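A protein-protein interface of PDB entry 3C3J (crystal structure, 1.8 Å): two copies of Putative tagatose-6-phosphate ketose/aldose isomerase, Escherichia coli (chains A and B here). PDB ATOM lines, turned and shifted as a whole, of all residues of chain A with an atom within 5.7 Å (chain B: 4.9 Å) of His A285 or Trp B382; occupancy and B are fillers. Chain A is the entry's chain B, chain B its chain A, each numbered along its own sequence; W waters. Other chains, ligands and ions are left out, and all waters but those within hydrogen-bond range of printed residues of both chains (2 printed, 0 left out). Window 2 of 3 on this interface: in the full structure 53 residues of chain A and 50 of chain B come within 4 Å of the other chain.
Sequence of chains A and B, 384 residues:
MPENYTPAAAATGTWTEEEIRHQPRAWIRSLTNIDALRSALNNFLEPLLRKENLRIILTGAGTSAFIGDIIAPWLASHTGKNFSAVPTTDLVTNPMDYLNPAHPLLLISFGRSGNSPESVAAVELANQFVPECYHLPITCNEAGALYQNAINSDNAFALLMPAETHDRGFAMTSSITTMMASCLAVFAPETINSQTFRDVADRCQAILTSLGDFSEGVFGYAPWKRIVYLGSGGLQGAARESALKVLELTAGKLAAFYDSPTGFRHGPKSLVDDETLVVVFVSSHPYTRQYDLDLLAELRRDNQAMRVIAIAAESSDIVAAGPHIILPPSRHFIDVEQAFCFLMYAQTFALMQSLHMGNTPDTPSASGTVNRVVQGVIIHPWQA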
ATOM      1  N   SER A 283     -21.389 -14.053 -18.186  1.00  0.00           N
ATOM      2  CA  SER A 283     -20.866 -13.987 -16.817  1.00  0.00           C
ATOM      3  C   SER A 283     -19.365 -13.685 -16.778  1.00  0.00           C
ATOM      4  O   SER A 283     -18.617 -14.092 -17.660  1.00  0.00           O
ATOM      5  CB  SER A 283     -21.112 -15.304 -16.094  1.00  0.00           C
ATOM      6  OG  SER A 283     -20.550 -15.320 -14.779  1.00  0.00           O
ATOM      7  N   SER A 284     -18.923 -13.031 -15.711  1.00  0.00           N
ATOM      8  CA  SER A 284     -17.493 -12.785 -15.483  1.00  0.00           C
ATOM      9  C   SER A 284     -16.859 -13.864 -14.586  1.00  0.00           C
ATOM     10  O   SER A 284     -15.666 -13.794 -14.275  1.00  0.00           O
ATOM     11  CB  SER A 284     -17.335 -11.436 -14.789  1.00  0.00           C
ATOM     12  OG  SER A 284     -18.004 -11.445 -13.543  1.00  0.00           O
ATOM     13  N   HIS A 285     -17.671 -14.817 -14.135  1.00  0.00           N
ATOM     14  CA  HIS A 285     -17.234 -15.912 -13.308  1.00  0.00           C
ATOM     15  C   HIS A 285     -16.856 -17.028 -14.276  1.00  0.00           C
ATOM     16  O   HIS A 285     -17.703 -17.561 -14.967  1.00  0.00           O
ATOM     17  CB  HIS A 285     -18.352 -16.324 -12.343  1.00  0.00           C
ATOM     18  CG  HIS A 285     -18.026 -17.502 -11.468  1.00  0.00           C
ATOM     19  ND1 HIS A 285     -16.901 -17.568 -10.681  1.00  0.00           N
ATOM     20  CD2 HIS A 285     -18.724 -18.636 -11.213  1.00  0.00           C
ATOM     21  CE1 HIS A 285     -16.906 -18.701 -10.000  1.00  0.00           C
ATOM     22  NE2 HIS A 285     -17.997 -19.373 -10.310  1.00  0.00           N
ATOM     23  N   PRO A 286     -15.563 -17.343 -14.371  1.00  0.00           N
ATOM     24  CA  PRO A 286     -15.149 -18.276 -15.417  1.00  0.00           C
ATOM     25  C   PRO A 286     -15.900 -19.613 -15.445  1.00  0.00           C
ATOM     26  O   PRO A 286     -16.256 -20.075 -16.528  1.00  0.00           O
ATOM     27  CB  PRO A 286     -13.649 -18.464 -15.121  1.00  0.00           C
ATOM     28  CG  PRO A 286     -13.265 -17.158 -14.598  1.00  0.00           C
ATOM     29  CD  PRO A 286     -14.394 -16.861 -13.627  1.00  0.00           C
ATOM     30  N   TYR A 287     -16.221 -20.179 -14.287  1.00  0.00           N
ATOM     31  CA  TYR A 287     -16.965 -21.446 -14.269  1.00  0.00           C
ATOM     32  C   TYR A 287     -18.332 -21.282 -14.963  1.00  0.00           C
ATOM     33  O   TYR A 287     -18.696 -22.052 -15.850  1.00  0.00           O
ATOM     34  CB  TYR A 287     -17.159 -21.985 -12.834  1.00  0.00           C
ATOM     35  CG  TYR A 287     -18.084 -23.190 -12.822  1.00  0.00           C
ATOM     36  CD1 TYR A 287     -17.618 -24.485 -13.117  1.00  0.00           C
ATOM     37  CD2 TYR A 287     -19.440 -23.029 -12.557  1.00  0.00           C
ATOM     38  CE1 TYR A 287     -18.509 -25.585 -13.103  1.00  0.00           C
ATOM     39  CE2 TYR A 287     -20.298 -24.080 -12.566  1.00  0.00           C
ATOM     40  CZ  TYR A 287     -19.849 -25.353 -12.850  1.00  0.00           C
ATOM     41  OH  TYR A 287     -20.793 -26.329 -12.849  1.00  0.00           O
ATOM     42  N   THR A 288     -19.065 -20.265 -14.558  1.00  0.00           N
ATOM     43  CA  THR A 288     -20.397 -19.950 -15.124  1.00  0.00           C
ATOM     44  C   THR A 288     -20.303 -19.573 -16.596  1.00  0.00           C
ATOM     45  O   THR A 288     -21.091 -20.033 -17.412  1.00  0.00           O
ATOM     46  CB  THR A 288     -21.009 -18.773 -14.359  1.00  0.00           C
ATOM     47  OG1 THR A 288     -20.977 -19.065 -12.949  1.00  0.00           O
ATOM     48  CG2 THR A 288     -22.469 -18.410 -14.843  1.00  0.00           C
ATOM     49  N   ARG A 289     -19.314 -18.746 -16.921  1.00  0.00           N
ATOM     50  CA  ARG A 289     -19.089 -18.233 -18.273  1.00  0.00           C
ATOM     51  C   ARG A 289     -18.966 -19.350 -19.296  1.00  0.00           C
ATOM     52  O   ARG A 289     -19.393 -19.184 -20.437  1.00  0.00           O
ATOM     53  CB  ARG A 289     -17.856 -17.318 -18.327  1.00  0.00           C
ATOM     54  CG  ARG A 289     -17.529 -16.772 -19.719  1.00  0.00           C
ATOM     55  CD  ARG A 289     -16.454 -15.658 -19.679  1.00  0.00           C
ATOM     56  NE  ARG A 289     -15.207 -16.218 -19.218  1.00  0.00           N
ATOM     57  CZ  ARG A 289     -14.225 -15.562 -18.593  1.00  0.00           C
ATOM     58  NH1 ARG A 289     -14.305 -14.254 -18.340  1.00  0.00           N
ATOM     59  NH2 ARG A 289     -13.123 -16.236 -18.224  1.00  0.00           N
ATOM     60  N   GLN A 290     -18.409 -20.487 -18.896  1.00  0.00           N
ATOM     61  CA  GLN A 290     -18.276 -21.629 -19.804  1.00  0.00           C
ATOM     62  C   GLN A 290     -19.638 -22.033 -20.386  1.00  0.00           C
ATOM     63  O   GLN A 290     -19.752 -22.308 -21.594  1.00  0.00           O
ATOM     64  CB  GLN A 290     -17.703 -22.831 -19.081  1.00  0.00           C
ATOM     65  CG  GLN A 290     -16.316 -22.684 -18.580  1.00  0.00           C
ATOM     66  CD  GLN A 290     -15.938 -23.871 -17.704  1.00  0.00           C
ATOM     67  OE1 GLN A 290     -16.537 -24.113 -16.624  1.00  0.00           O
ATOM     68  NE2 GLN A 290     -14.954 -24.612 -18.150  1.00  0.00           N
ATOM     69  N   HIS A 332     -11.676  -6.577 -12.588  1.00  0.00           N
ATOM     70  CA  HIS A 332     -12.636  -7.658 -12.536  1.00  0.00           C
ATOM     71  C   HIS A 332     -13.874  -7.213 -11.767  1.00  0.00           C
ATOM     72  O   HIS A 332     -13.745  -6.710 -10.645  1.00  0.00           O
ATOM     73  CB  HIS A 332     -12.055  -8.875 -11.817  1.00  0.00           C
ATOM     74  CG  HIS A 332     -13.017 -10.022 -11.755  1.00  0.00           C
ATOM     75  ND1 HIS A 332     -13.363 -10.749 -12.870  1.00  0.00           N
ATOM     76  CD2 HIS A 332     -13.772 -10.503 -10.740  1.00  0.00           C
ATOM     77  CE1 HIS A 332     -14.254 -11.667 -12.531  1.00  0.00           C
ATOM     78  NE2 HIS A 332     -14.530 -11.530 -11.247  1.00  0.00           N
ATOM     79  N   ASP A 335     -20.643 -10.628 -10.810  1.00  0.00           N
ATOM     80  CA  ASP A 335     -21.854 -10.541 -11.628  1.00  0.00           C
ATOM     81  C   ASP A 335     -22.894  -9.496 -11.162  1.00  0.00           C
ATOM     82  O   ASP A 335     -23.539  -8.866 -12.000  1.00  0.00           O
ATOM     83  CB  ASP A 335     -22.472 -11.915 -11.856  1.00  0.00           C
ATOM     84  CG  ASP A 335     -21.801 -12.701 -13.013  1.00  0.00           C
ATOM     85  OD1 ASP A 335     -21.141 -12.096 -13.909  1.00  0.00           O
ATOM     86  OD2 ASP A 335     -21.950 -13.952 -13.029  1.00  0.00           O
ATOM     87  N   PRO B  95     -23.697 -22.920  -8.661  1.00  0.00           N
ATOM     88  CA  PRO B  95     -23.936 -23.722  -7.450  1.00  0.00           C
ATOM     89  C   PRO B  95     -23.674 -22.966  -6.156  1.00  0.00           C
ATOM     90  O   PRO B  95     -24.395 -23.157  -5.180  1.00  0.00           O
ATOM     91  CB  PRO B  95     -22.925 -24.870  -7.563  1.00  0.00           C
ATOM     92  CG  PRO B  95     -21.920 -24.431  -8.554  1.00  0.00           C
ATOM     93  CD  PRO B  95     -22.669 -23.532  -9.515  1.00  0.00           C
ATOM     94  N   MET B  96     -22.655 -22.106  -6.166  1.00  0.00           N
ATOM     95  CA  MET B  96     -22.278 -21.343  -4.969  1.00  0.00           C
ATOM     96  C   MET B  96     -23.365 -20.380  -4.495  1.00  0.00           C
ATOM     97  O   MET B  96     -23.395 -20.003  -3.325  1.00  0.00           O
ATOM     98  CB  MET B  96     -20.964 -20.578  -5.218  1.00  0.00           C
ATOM     99  CG  MET B  96     -21.005 -19.510  -6.345  1.00  0.00           C
ATOM    100  SD  MET B  96     -21.045 -20.128  -8.280  1.00  0.00           S
ATOM    101  CE  MET B  96     -21.474 -18.355  -9.144  1.00  0.00           C
ATOM    102  N   LEU B 125     -22.996 -31.814  -7.597  1.00  0.00           N
ATOM    103  CA  LEU B 125     -22.663 -30.512  -7.039  1.00  0.00           C
ATOM    104  C   LEU B 125     -23.205 -30.351  -5.610  1.00  0.00           C
ATOM    105  O   LEU B 125     -22.485 -29.871  -4.723  1.00  0.00           O
ATOM    106  CB  LEU B 125     -23.170 -29.424  -7.977  1.00  0.00           C
ATOM    107  CG  LEU B 125     -22.325 -29.129  -9.223  1.00  0.00           C
ATOM    108  CD1 LEU B 125     -23.175 -28.297 -10.227  1.00  0.00           C
ATOM    109  CD2 LEU B 125     -21.038 -28.381  -8.831  1.00  0.00           C
ATOM    110  N   GLN B 128     -20.954 -32.352  -3.433  1.00  0.00           N
ATOM    111  CA  GLN B 128     -19.683 -31.634  -3.304  1.00  0.00           C
ATOM    112  C   GLN B 128     -19.773 -30.435  -2.356  1.00  0.00           C
ATOM    113  O   GLN B 128     -18.870 -30.226  -1.531  1.00  0.00           O
ATOM    114  CB  GLN B 128     -19.214 -31.132  -4.663  1.00  0.00           C
ATOM    115  CG  GLN B 128     -18.495 -32.117  -5.530  1.00  0.00           C
ATOM    116  CD  GLN B 128     -18.033 -31.427  -6.828  1.00  0.00           C
ATOM    117  OE1 GLN B 128     -16.876 -30.978  -6.959  1.00  0.00           O
ATOM    118  NE2 GLN B 128     -18.947 -31.283  -7.744  1.00  0.00           N
ATOM    119  N   PHE B 129     -20.840 -29.644  -2.489  1.00  0.00           N
ATOM    120  CA  PHE B 129     -20.985 -28.399  -1.718  1.00  0.00           C
ATOM    121  C   PHE B 129     -21.498 -28.587  -0.279  1.00  0.00           C
ATOM    122  O   PHE B 129     -21.094 -27.848   0.614  1.00  0.00           O
ATOM    123  CB  PHE B 129     -21.905 -27.400  -2.433  1.00  0.00           C
ATOM    124  CG  PHE B 129     -21.203 -26.540  -3.444  1.00  0.00           C
ATOM    125  CD1 PHE B 129     -20.769 -27.059  -4.632  1.00  0.00           C
ATOM    126  CD2 PHE B 129     -20.986 -25.184  -3.198  1.00  0.00           C
ATOM    127  CE1 PHE B 129     -20.101 -26.242  -5.553  1.00  0.00           C
ATOM    128  CE2 PHE B 129     -20.322 -24.391  -4.105  1.00  0.00           C
ATOM    129  CZ  PHE B 129     -19.897 -24.914  -5.281  1.00  0.00           C
ATOM    130  N   HIS B 380     -19.317 -28.982 -17.096  1.00  0.00           N
ATOM    131  CA  HIS B 380     -17.957 -28.642 -16.752  1.00  0.00           C
ATOM    132  C   HIS B 380     -17.764 -28.872 -15.269  1.00  0.00           C
ATOM    133  O   HIS B 380     -18.662 -28.637 -14.479  1.00  0.00           O
ATOM    134  CB  HIS B 380     -17.656 -27.195 -17.101  1.00  0.00           C
ATOM    135  CG  HIS B 380     -17.762 -26.898 -18.560  1.00  0.00           C
ATOM    136  ND1 HIS B 380     -18.895 -26.354 -19.131  1.00  0.00           N
ATOM    137  CD2 HIS B 380     -16.891 -27.105 -19.576  1.00  0.00           C
ATOM    138  CE1 HIS B 380     -18.705 -26.220 -20.432  1.00  0.00           C
ATOM    139  NE2 HIS B 380     -17.498 -26.663 -20.727  1.00  0.00           N
ATOM    140  N   PRO B 381     -16.593 -29.357 -14.892  1.00  0.00           N
ATOM    141  CA  PRO B 381     -16.363 -29.685 -13.496  1.00  0.00           C
ATOM    142  C   PRO B 381     -16.138 -28.432 -12.658  1.00  0.00           C
ATOM    143  O   PRO B 381     -15.513 -27.498 -13.126  1.00  0.00           O
ATOM    144  CB  PRO B 381     -15.096 -30.540 -13.557  1.00  0.00           C
ATOM    145  CG  PRO B 381     -14.345 -30.016 -14.741  1.00  0.00           C
ATOM    146  CD  PRO B 381     -15.414 -29.624 -15.737  1.00  0.00           C
ATOM    147  N   TRP B 382     -16.657 -28.415 -11.437  1.00  0.00           N
ATOM    148  CA  TRP B 382     -16.408 -27.315 -10.523  1.00  0.00           C
ATOM    149  C   TRP B 382     -14.915 -27.243 -10.207  1.00  0.00           C
ATOM    150  O   TRP B 382     -14.350 -26.164 -10.131  1.00  0.00           O
ATOM    151  CB  TRP B 382     -17.186 -27.507  -9.233  1.00  0.00           C
ATOM    152  CG  TRP B 382     -17.012 -26.403  -8.256  1.00  0.00           C
ATOM    153  CD1 TRP B 382     -16.387 -26.483  -7.048  1.00  0.00           C
ATOM    154  CD2 TRP B 382     -17.480 -25.053  -8.376  1.00  0.00           C
ATOM    155  NE1 TRP B 382     -16.432 -25.265  -6.406  1.00  0.00           N
ATOM    156  CE2 TRP B 382     -17.105 -24.374  -7.189  1.00  0.00           C
ATOM    157  CE3 TRP B 382     -18.210 -24.362  -9.346  1.00  0.00           C
ATOM    158  CZ2 TRP B 382     -17.397 -23.030  -6.969  1.00  0.00           C
ATOM    159  CZ3 TRP B 382     -18.517 -23.029  -9.117  1.00  0.00           C
ATOM    160  CH2 TRP B 382     -18.114 -22.379  -7.933  1.00  0.00           C
ATOM    161  N   GLN B 383     -14.291 -28.386  -9.979  1.00  0.00           N
ATOM    162  CA  GLN B 383     -12.831 -28.436  -9.869  1.00  0.00           C
ATOM    163  C   GLN B 383     -12.157 -28.350 -11.258  1.00  0.00           C
ATOM    164  O   GLN B 383     -12.133 -29.336 -12.010  1.00  0.00           O
ATOM    165  CB  GLN B 383     -12.393 -29.708  -9.125  1.00  0.00           C
ATOM    166  CG  GLN B 383     -10.880 -29.944  -9.154  1.00  0.00           C
ATOM    167  CD  GLN B 383     -10.101 -28.868  -8.409  1.00  0.00           C
ATOM    168  OE1 GLN B 383     -10.218 -28.738  -7.161  1.00  0.00           O
ATOM    169  NE2 GLN B 383      -9.283 -28.103  -9.160  1.00  0.00           N
ATOM    170  N   ALA B 384     -11.597 -27.183 -11.583  1.00  0.00           N
ATOM    171  CA  ALA B 384     -10.951 -26.984 -12.875  1.00  0.00           C
ATOM    172  C   ALA B 384      -9.759 -27.911 -12.999  1.00  0.00           C
ATOM    173  O   ALA B 384      -9.463 -28.410 -14.096  1.00  0.00           O
ATOM    174  CB  ALA B 384     -10.507 -25.561 -13.054  1.00  0.00           C
HETATM  175  O   HOH W   1     -20.009 -29.498 -12.234  1.00  0.00           O
HETATM  176  O   HOH W   2     -14.697 -26.018 -15.192  1.00  0.00           O
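Among the printed residues, merely in contact across the chains: Gln A290 with His B380, Tyr A287 with His B380, Tyr A287 with Pro B381, Tyr A287 with Trp B382, His A285 with Trp B382, Thr A288 with Met B96 and Tyr A287 with Pro B95.
A ring nitrogen (NE2) of His A285 sits at hydrogen-bond distance from the side-chain sulfur of Met B96 (3.7 Å).
Water W2 lies within hydrogen-bond range of the backbone carbonyl oxygen of Pro B381 (2.7 Å) and the side-chain amide oxygen of Gln A290 (3.0 Å).
Water W1 lies within hydrogen-bond range of the backbone carbonyl oxygen (O) of His B380 (2.8 Å) and the side-chain hydroxyl (OH) of Tyr A287 (3.3 Å).
The side-chain hydroxyl (OG) of Ser A283 is in hydrogen-bond range of the backbone NH (N) of His A285, at 3.0 Å.
OE1 of Gln A290 lies close to O of Tyr A287 (3.1 Å).
No position is printed for both chains.
Of the 10 printed residues of chain A, 4 touch a printed residue of chain B.
Along chain A the printed residues that touch a printed residue of chain B span positions 285 to 290.
Among the printed residues, 8 pairs touch across the chains.
Among the printed residues, no Asp or Glu carboxylate lies within 4 Å of a Lys or Arg side-chain nitrogen of the other chain.
His A285 touches just these residues of chain B: Met B96 (3.5 Å) and Trp B382 (3.8 Å).
Printed residues of chain B within 4 Å of Tyr A287: Pro B95 (3.9 Å), His B380 (3.4 Å), Pro B381 (3.6 Å) and Trp B382 (3.6 Å).
Printed residues of chain B within 4 Å of Thr A288: Met B96 (3.9 Å).
Of the printed residues of chain A, Met B96 touches His A285 and Thr A288.
Phe B129 touches none of the printed residues of chain A.
Of the printed residues of chain A, His B380 touches Tyr A287 (3.4 Å) and Gln A290 (3.3 Å).
Of the printed residues of chain A, Pro B381 touches Tyr A287.
Of chain A, only His A285 and Tyr A287 come within 4 Å of Trp B382.
The nearest printed residue of chain A that does not touch Trp B382 is Thr A288 (6.0 Å).
The nearest printed residue of chain A that does not touch His B380 is Thr A288 (6.9 Å).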
